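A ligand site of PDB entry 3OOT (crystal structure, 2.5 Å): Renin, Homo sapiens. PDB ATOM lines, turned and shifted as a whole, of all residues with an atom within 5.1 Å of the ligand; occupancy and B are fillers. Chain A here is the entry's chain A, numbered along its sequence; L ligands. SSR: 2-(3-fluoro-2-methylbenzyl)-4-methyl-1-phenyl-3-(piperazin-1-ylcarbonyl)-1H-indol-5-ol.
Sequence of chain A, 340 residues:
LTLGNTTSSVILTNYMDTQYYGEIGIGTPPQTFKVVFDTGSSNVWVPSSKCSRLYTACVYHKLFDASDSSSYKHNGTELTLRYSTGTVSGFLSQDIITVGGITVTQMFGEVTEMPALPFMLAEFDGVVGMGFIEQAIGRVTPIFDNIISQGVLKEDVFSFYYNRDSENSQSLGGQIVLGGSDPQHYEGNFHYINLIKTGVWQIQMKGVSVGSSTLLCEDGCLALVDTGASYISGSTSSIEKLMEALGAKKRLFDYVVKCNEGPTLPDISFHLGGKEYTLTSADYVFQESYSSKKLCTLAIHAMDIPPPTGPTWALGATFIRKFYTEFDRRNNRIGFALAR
The backbone NH (N) of Thr 85 sits at hydrogen-bond distance from an oxygen (O32) of the ligand, at 3.3 Å.
N21 of the ligand is in salt-bridge range of OD2 of Asp 226 (2.9 Å).
A ring nitrogen (NE2) of His 301 lies within hydrogen-bond range of an oxygen (O16) of the ligand, at 2.6 Å.
OD1 of Asp 38 lies within salt-bridge range of N21 of the ligand (2.9 Å).
An oxygen (O32) of the ligand lies within hydrogen-bond range of the side-chain hydroxyl of Thr 85 (2.8 Å).
The side-chain carboxylate of Asp 226 lies within hydrogen-bond range of the backbone NH of Ala 229 (3.2 Å).
OG of Ser 41 sits at hydrogen-bond distance from OD2 of Asp 38 (2.6 Å).
The side-chain hydroxyl (OG) of Ser 230 lies within hydrogen-bond range of the backbone carbonyl oxygen (O) of Thr 18, at 2.5 Å.
The backbone carbonyl oxygen (O) of Leu 121 lies within hydrogen-bond range of the side-chain amide nitrogen (NE2) of Gln 19, 3.1 Å away.
OD1 of Asp 226 sits at hydrogen-bond distance from N of Gly 228 (3.0 Å).
N of Gly 40 lies within hydrogen-bond range of OD1 of Asp 38 (2.9 Å).
Merely in contact with the ligand: Gly 228, Val 36, Val 127, Tyr 83, Gln 19, Ser 230, Ala 229, Phe 124 and Ser 84.
Hydrophobic or aromatic side chains within 4 Å of the ligand: Val 36, Tyr 83, Phe 124, Val 127 and His 301.
Within 4 Å of the ligand: Gln 19, Val 36, Asp 38, Tyr 83, Ser 84, Thr 85, Phe 124, Val 127, Asp 226, Gly 228, Ala 229, Ser 230 and His 301.
The nearest printed residue that does not touch the ligand is Pro 118 (4.01 Å).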
ATOM      1  N   THR A  18      23.543 -14.655   6.541  1.00  0.00           N
ATOM      2  CA  THR A  18      23.068 -14.057   5.291  1.00  0.00           C
ATOM      3  C   THR A  18      23.932 -14.429   4.070  1.00  0.00           C
ATOM      4  O   THR A  18      23.460 -14.329   2.927  1.00  0.00           O
ATOM      5  CB  THR A  18      22.960 -12.543   5.413  1.00  0.00           C
ATOM      6  OG1 THR A  18      24.241 -12.012   5.724  1.00  0.00           O
ATOM      7  CG2 THR A  18      21.948 -12.091   6.449  1.00  0.00           C
ATOM      8  N   GLN A  19      25.193 -14.853   4.299  1.00  0.00           N
ATOM      9  CA  GLN A  19      26.109 -15.195   3.208  1.00  0.00           C
ATOM     10  C   GLN A  19      26.828 -16.470   3.558  1.00  0.00           C
ATOM     11  O   GLN A  19      27.443 -16.550   4.606  1.00  0.00           O
ATOM     12  CB  GLN A  19      27.128 -14.058   2.958  1.00  0.00           C
ATOM     13  CG  GLN A  19      26.537 -12.760   2.403  1.00  0.00           C
ATOM     14  CD  GLN A  19      27.504 -11.600   2.390  1.00  0.00           C
ATOM     15  OE1 GLN A  19      28.618 -11.709   1.904  1.00  0.00           O
ATOM     16  NE2 GLN A  19      27.086 -10.442   2.912  1.00  0.00           N
ATOM     17  N   VAL A  36      29.799 -17.643  -3.763  1.00  0.00           N
ATOM     18  CA  VAL A  36      28.474 -18.109  -3.354  1.00  0.00           C
ATOM     19  C   VAL A  36      28.031 -19.126  -4.429  1.00  0.00           C
ATOM     20  O   VAL A  36      28.221 -18.898  -5.633  1.00  0.00           O
ATOM     21  CB  VAL A  36      27.466 -16.939  -3.146  1.00  0.00           C
ATOM     22  CG1 VAL A  36      26.046 -17.445  -3.000  1.00  0.00           C
ATOM     23  CG2 VAL A  36      27.816 -16.172  -1.897  1.00  0.00           C
ATOM     24  N   ASP A  38      25.119 -20.473  -6.107  1.00  0.00           N
ATOM     25  CA  ASP A  38      23.772 -19.968  -6.369  1.00  0.00           C
ATOM     26  C   ASP A  38      22.917 -20.794  -7.352  1.00  0.00           C
ATOM     27  O   ASP A  38      23.199 -20.821  -8.537  1.00  0.00           O
ATOM     28  CB  ASP A  38      23.920 -18.493  -6.827  1.00  0.00           C
ATOM     29  CG  ASP A  38      22.652 -17.783  -7.237  1.00  0.00           C
ATOM     30  OD1 ASP A  38      21.584 -18.098  -6.683  1.00  0.00           O
ATOM     31  OD2 ASP A  38      22.753 -16.863  -8.065  1.00  0.00           O
ATOM     32  N   GLY A  40      19.885 -19.952  -8.036  1.00  0.00           N
ATOM     33  CA  GLY A  40      19.049 -18.919  -8.648  1.00  0.00           C
ATOM     34  C   GLY A  40      19.651 -18.253  -9.868  1.00  0.00           C
ATOM     35  O   GLY A  40      19.081 -17.296 -10.384  1.00  0.00           O
ATOM     36  N   SER A  41      20.835 -18.746 -10.334  1.00  0.00           N
ATOM     37  CA  SER A  41      21.564 -18.243 -11.517  1.00  0.00           C
ATOM     38  C   SER A  41      22.455 -19.365 -12.118  1.00  0.00           C
ATOM     39  O   SER A  41      22.640 -20.379 -11.457  1.00  0.00           O
ATOM     40  CB  SER A  41      22.340 -16.961 -11.216  1.00  0.00           C
ATOM     41  OG  SER A  41      23.566 -17.191 -10.523  1.00  0.00           O
ATOM     42  N   TYR A  83      20.647  -9.140 -11.903  1.00  0.00           N
ATOM     43  CA  TYR A  83      20.122  -9.878 -10.765  1.00  0.00           C
ATOM     44  C   TYR A  83      19.126  -8.984 -10.056  1.00  0.00           C
ATOM     45  O   TYR A  83      19.091  -7.772 -10.334  1.00  0.00           O
ATOM     46  CB  TYR A  83      21.241 -10.245  -9.788  1.00  0.00           C
ATOM     47  CG  TYR A  83      22.344 -11.084 -10.391  1.00  0.00           C
ATOM     48  CD1 TYR A  83      22.160 -12.447 -10.627  1.00  0.00           C
ATOM     49  CD2 TYR A  83      23.597 -10.541 -10.638  1.00  0.00           C
ATOM     50  CE1 TYR A  83      23.176 -13.244 -11.138  1.00  0.00           C
ATOM     51  CE2 TYR A  83      24.633 -11.318 -11.158  1.00  0.00           C
ATOM     52  CZ  TYR A  83      24.415 -12.675 -11.390  1.00  0.00           C
ATOM     53  OH  TYR A  83      25.449 -13.460 -11.870  1.00  0.00           O
ATOM     54  N   SER A  84      18.337  -9.563  -9.139  1.00  0.00           N
ATOM     55  CA  SER A  84      17.310  -8.855  -8.387  1.00  0.00           C
ATOM     56  C   SER A  84      17.856  -7.654  -7.601  1.00  0.00           C
ATOM     57  O   SER A  84      17.178  -6.622  -7.533  1.00  0.00           O
ATOM     58  CB  SER A  84      16.600  -9.806  -7.440  1.00  0.00           C
ATOM     59  OG  SER A  84      15.974 -10.857  -8.168  1.00  0.00           O
ATOM     60  N   THR A  85      19.092  -7.794  -7.036  1.00  0.00           N
ATOM     61  CA  THR A  85      19.727  -6.773  -6.202  1.00  0.00           C
ATOM     62  C   THR A  85      20.706  -5.834  -6.894  1.00  0.00           C
ATOM     63  O   THR A  85      21.123  -4.837  -6.290  1.00  0.00           O
ATOM     64  CB  THR A  85      20.405  -7.429  -5.002  1.00  0.00           C
ATOM     65  OG1 THR A  85      21.445  -8.299  -5.463  1.00  0.00           O
ATOM     66  CG2 THR A  85      19.424  -8.133  -4.084  1.00  0.00           C
ATOM     67  N   GLY A  86      21.113  -6.159  -8.104  1.00  0.00           N
ATOM     68  CA  GLY A  86      22.070  -5.355  -8.839  1.00  0.00           C
ATOM     69  C   GLY A  86      22.555  -6.011 -10.117  1.00  0.00           C
ATOM     70  O   GLY A  86      22.120  -7.123 -10.454  1.00  0.00           O
ATOM     71  N   PRO A 118      25.030  -3.603  -4.629  1.00  0.00           N
ATOM     72  CA  PRO A 118      25.280  -4.175  -3.291  1.00  0.00           C
ATOM     73  C   PRO A 118      26.652  -4.800  -3.042  1.00  0.00           C
ATOM     74  O   PRO A 118      26.897  -5.256  -1.922  1.00  0.00           O
ATOM     75  CB  PRO A 118      24.194  -5.270  -3.231  1.00  0.00           C
ATOM     76  CG  PRO A 118      24.149  -5.798  -4.653  1.00  0.00           C
ATOM     77  CD  PRO A 118      24.495  -4.618  -5.551  1.00  0.00           C
ATOM     78  N   PHE A 119      27.512  -4.860  -4.061  1.00  0.00           N
ATOM     79  CA  PHE A 119      28.764  -5.619  -4.017  1.00  0.00           C
ATOM     80  C   PHE A 119      29.811  -5.271  -2.992  1.00  0.00           C
ATOM     81  O   PHE A 119      30.588  -6.144  -2.617  1.00  0.00           O
ATOM     82  CB  PHE A 119      29.304  -5.912  -5.406  1.00  0.00           C
ATOM     83  CG  PHE A 119      28.306  -6.677  -6.224  1.00  0.00           C
ATOM     84  CD1 PHE A 119      28.075  -8.026  -5.995  1.00  0.00           C
ATOM     85  CD2 PHE A 119      27.520  -6.027  -7.175  1.00  0.00           C
ATOM     86  CE1 PHE A 119      27.120  -8.734  -6.733  1.00  0.00           C
ATOM     87  CE2 PHE A 119      26.571  -6.737  -7.906  1.00  0.00           C
ATOM     88  CZ  PHE A 119      26.379  -8.099  -7.687  1.00  0.00           C
ATOM     89  N   LEU A 121      28.974  -4.838   0.070  1.00  0.00           N
ATOM     90  CA  LEU A 121      28.414  -5.549   1.221  1.00  0.00           C
ATOM     91  C   LEU A 121      28.686  -7.046   1.153  1.00  0.00           C
ATOM     92  O   LEU A 121      28.477  -7.750   2.143  1.00  0.00           O
ATOM     93  CB  LEU A 121      26.909  -5.294   1.304  1.00  0.00           C
ATOM     94  CG  LEU A 121      26.469  -3.818   1.418  1.00  0.00           C
ATOM     95  CD1 LEU A 121      24.947  -3.729   1.580  1.00  0.00           C
ATOM     96  CD2 LEU A 121      27.181  -3.129   2.563  1.00  0.00           C
ATOM     97  N   ALA A 122      29.118  -7.538  -0.017  1.00  0.00           N
ATOM     98  CA  ALA A 122      29.423  -8.933  -0.260  1.00  0.00           C
ATOM     99  C   ALA A 122      30.753  -9.300   0.361  1.00  0.00           C
ATOM    100  O   ALA A 122      31.751  -8.603   0.136  1.00  0.00           O
ATOM    101  CB  ALA A 122      29.461  -9.211  -1.762  1.00  0.00           C
ATOM    102  N   PHE A 124      31.782 -12.387  -0.260  1.00  0.00           N
ATOM    103  CA  PHE A 124      32.213 -13.200  -1.394  1.00  0.00           C
ATOM    104  C   PHE A 124      32.746 -12.274  -2.525  1.00  0.00           C
ATOM    105  O   PHE A 124      32.329 -11.116  -2.645  1.00  0.00           O
ATOM    106  CB  PHE A 124      31.047 -14.078  -1.879  1.00  0.00           C
ATOM    107  CG  PHE A 124      29.797 -13.318  -2.301  1.00  0.00           C
ATOM    108  CD1 PHE A 124      28.804 -13.016  -1.379  1.00  0.00           C
ATOM    109  CD2 PHE A 124      29.608 -12.930  -3.621  1.00  0.00           C
ATOM    110  CE1 PHE A 124      27.643 -12.345  -1.775  1.00  0.00           C
ATOM    111  CE2 PHE A 124      28.472 -12.220  -4.011  1.00  0.00           C
ATOM    112  CZ  PHE A 124      27.484 -11.954  -3.093  1.00  0.00           C
ATOM    113  N   VAL A 127      30.489 -15.407  -7.889  1.00  0.00           N
ATOM    114  CA  VAL A 127      29.325 -16.279  -7.886  1.00  0.00           C
ATOM    115  C   VAL A 127      29.570 -17.509  -8.767  1.00  0.00           C
ATOM    116  O   VAL A 127      30.213 -17.399  -9.808  1.00  0.00           O
ATOM    117  CB  VAL A 127      28.091 -15.445  -8.366  1.00  0.00           C
ATOM    118  CG1 VAL A 127      26.885 -16.339  -8.694  1.00  0.00           C
ATOM    119  CG2 VAL A 127      27.727 -14.391  -7.330  1.00  0.00           C
ATOM    120  N   ASP A 226      16.375 -20.860  -4.020  1.00  0.00           N
ATOM    121  CA  ASP A 226      17.578 -20.045  -4.262  1.00  0.00           C
ATOM    122  C   ASP A 226      18.561 -20.054  -3.072  1.00  0.00           C
ATOM    123  O   ASP A 226      18.349 -19.364  -2.084  1.00  0.00           O
ATOM    124  CB  ASP A 226      17.143 -18.618  -4.616  1.00  0.00           C
ATOM    125  CG  ASP A 226      18.210 -17.703  -5.158  1.00  0.00           C
ATOM    126  OD1 ASP A 226      19.403 -17.943  -4.870  1.00  0.00           O
ATOM    127  OD2 ASP A 226      17.859 -16.723  -5.822  1.00  0.00           O
ATOM    128  N   GLY A 228      21.515 -18.734  -2.948  1.00  0.00           N
ATOM    129  CA  GLY A 228      22.193 -17.446  -2.850  1.00  0.00           C
ATOM    130  C   GLY A 228      21.384 -16.362  -2.169  1.00  0.00           C
ATOM    131  O   GLY A 228      21.954 -15.369  -1.691  1.00  0.00           O
ATOM    132  N   ALA A 229      20.051 -16.518  -2.100  1.00  0.00           N
ATOM    133  CA  ALA A 229      19.194 -15.552  -1.448  1.00  0.00           C
ATOM    134  C   ALA A 229      19.358 -15.682   0.072  1.00  0.00           C
ATOM    135  O   ALA A 229      19.276 -16.792   0.619  1.00  0.00           O
ATOM    136  CB  ALA A 229      17.735 -15.796  -1.855  1.00  0.00           C
ATOM    137  N   SER A 230      19.604 -14.545   0.769  1.00  0.00           N
ATOM    138  CA  SER A 230      19.801 -14.522   2.219  1.00  0.00           C
ATOM    139  C   SER A 230      18.568 -14.877   2.990  1.00  0.00           C
ATOM    140  O   SER A 230      18.656 -15.490   4.054  1.00  0.00           O
ATOM    141  CB  SER A 230      20.242 -13.138   2.664  1.00  0.00           C
ATOM    142  OG  SER A 230      21.532 -12.847   2.167  1.00  0.00           O
ATOM    143  N   TYR A 231      17.398 -14.396   2.492  1.00  0.00           N
ATOM    144  CA  TYR A 231      16.116 -14.505   3.132  1.00  0.00           C
ATOM    145  C   TYR A 231      15.115 -15.246   2.270  1.00  0.00           C
ATOM    146  O   TYR A 231      15.395 -15.556   1.109  1.00  0.00           O
ATOM    147  CB  TYR A 231      15.567 -13.076   3.328  1.00  0.00           C
ATOM    148  CG  TYR A 231      16.306 -12.170   4.277  1.00  0.00           C
ATOM    149  CD1 TYR A 231      15.878 -10.858   4.502  1.00  0.00           C
ATOM    150  CD2 TYR A 231      17.369 -12.642   5.058  1.00  0.00           C
ATOM    151  CE1 TYR A 231      16.539 -10.022   5.399  1.00  0.00           C
ATOM    152  CE2 TYR A 231      18.062 -11.807   5.926  1.00  0.00           C
ATOM    153  CZ  TYR A 231      17.640 -10.494   6.104  1.00  0.00           C
ATOM    154  OH  TYR A 231      18.291  -9.669   6.991  1.00  0.00           O
ATOM    155  N   SER A 233      11.838 -14.686   0.266  1.00  0.00           N
ATOM    156  CA  SER A 233      11.223 -13.507  -0.366  1.00  0.00           C
ATOM    157  C   SER A 233       9.905 -13.849  -1.047  1.00  0.00           C
ATOM    158  O   SER A 233       9.686 -14.978  -1.473  1.00  0.00           O
ATOM    159  CB  SER A 233      12.170 -12.815  -1.342  1.00  0.00           C
ATOM    160  OG  SER A 233      12.398 -13.573  -2.523  1.00  0.00           O
ATOM    161  N   HIS A 301      11.788 -10.876   3.284  1.00  0.00           N
ATOM    162  CA  HIS A 301      11.643  -9.549   2.673  1.00  0.00           C
ATOM    163  C   HIS A 301      10.945  -9.575   1.312  1.00  0.00           C
ATOM    164  O   HIS A 301      10.606 -10.644   0.807  1.00  0.00           O
ATOM    165  CB  HIS A 301      12.963  -8.747   2.686  1.00  0.00           C
ATOM    166  CG  HIS A 301      14.022  -9.241   1.745  1.00  0.00           C
ATOM    167  ND1 HIS A 301      15.216  -8.540   1.610  1.00  0.00           N
ATOM    168  CD2 HIS A 301      14.066 -10.334   0.956  1.00  0.00           C
ATOM    169  CE1 HIS A 301      15.927  -9.220   0.720  1.00  0.00           C
ATOM    170  NE2 HIS A 301      15.272 -10.310   0.297  1.00  0.00           N
ATOM    171  N   MET A 303      10.649  -9.109  -2.812  1.00  0.00           N
ATOM    172  CA  MET A 303      11.441  -9.161  -4.033  1.00  0.00           C
ATOM    173  C   MET A 303      10.540  -9.419  -5.213  1.00  0.00           C
ATOM    174  O   MET A 303       9.918 -10.487  -5.295  1.00  0.00           O
ATOM    175  CB  MET A 303      12.547 -10.219  -4.008  1.00  0.00           C
ATOM    176  CG  MET A 303      13.890  -9.721  -3.586  1.00  0.00           C
ATOM    177  SD  MET A 303      14.630  -8.452  -4.610  1.00  0.00           S
ATOM    178  CE  MET A 303      15.777  -7.800  -3.438  1.00  0.00           C
HETATM  179  C1  SSR L   1      18.768 -11.160  -0.403  1.00  0.00           C
HETATM  180  C2  SSR L   1      20.113 -10.803  -0.577  1.00  0.00           C
HETATM  181  C3  SSR L   1      20.712 -10.882  -1.843  1.00  0.00           C
HETATM  182  C4  SSR L   1      19.939 -11.327  -2.942  1.00  0.00           C
HETATM  183  C5  SSR L   1      18.571 -11.678  -2.773  1.00  0.00           C
HETATM  184  C6  SSR L   1      17.990 -11.568  -1.498  1.00  0.00           C
HETATM  185  N9  SSR L   1      21.985 -10.811  -2.281  1.00  0.00           N
HETATM  186  C10 SSR L   1      22.168 -10.913  -3.627  1.00  0.00           C
HETATM  187  C11 SSR L   1      20.944 -11.386  -4.065  1.00  0.00           C
HETATM  188  C12 SSR L   1      17.676 -12.012  -3.945  1.00  0.00           C
HETATM  189  O16 SSR L   1      16.678 -11.874  -1.278  1.00  0.00           O
HETATM  190  C17 SSR L   1      20.492 -11.681  -5.454  1.00  0.00           C
HETATM  191  N18 SSR L   1      20.179 -12.946  -5.803  1.00  0.00           N
HETATM  192  C19 SSR L   1      20.269 -14.049  -4.823  1.00  0.00           C
HETATM  193  C20 SSR L   1      20.972 -15.226  -5.484  1.00  0.00           C
HETATM  194  N21 SSR L   1      20.348 -15.528  -6.748  1.00  0.00           N
HETATM  195  C22 SSR L   1      20.294 -14.481  -7.739  1.00  0.00           C
HETATM  196  C23 SSR L   1      19.665 -13.222  -7.156  1.00  0.00           C
HETATM  197  O32 SSR L   1      20.445 -10.753  -6.257  1.00  0.00           O
HETATM  198  C35 SSR L   1      22.945 -10.279  -1.472  1.00  0.00           C
HETATM  199  C36 SSR L   1      23.554  -9.022  -1.713  1.00  0.00           C
HETATM  200  C37 SSR L   1      24.568  -8.514  -0.907  1.00  0.00           C
HETATM  201  C38 SSR L   1      24.987  -9.219   0.230  1.00  0.00           C
HETATM  202  C39 SSR L   1      24.407 -10.449   0.524  1.00  0.00           C
HETATM  203  C40 SSR L   1      23.422 -10.961  -0.324  1.00  0.00           C
HETATM  204  C46 SSR L   1      23.437 -10.722  -4.450  1.00  0.00           C
HETATM  205  C47 SSR L   1      23.730 -11.911  -5.331  1.00  0.00           C
HETATM  206  C50 SSR L   1      24.056 -13.200  -4.827  1.00  0.00           C
HETATM  207  C51 SSR L   1      24.351 -14.218  -5.718  1.00  0.00           C
HETATM  208  C52 SSR L   1      24.280 -13.992  -7.106  1.00  0.00           C
HETATM  209  C53 SSR L   1      23.972 -12.715  -7.602  1.00  0.00           C
HETATM  210  C54 SSR L   1      23.728 -11.671  -6.706  1.00  0.00           C
HETATM  211  C58 SSR L   1      24.131 -13.547  -3.348  1.00  0.00           C
HETATM  212  F62 SSR L   1      24.674 -15.428  -5.239  1.00  0.00           F
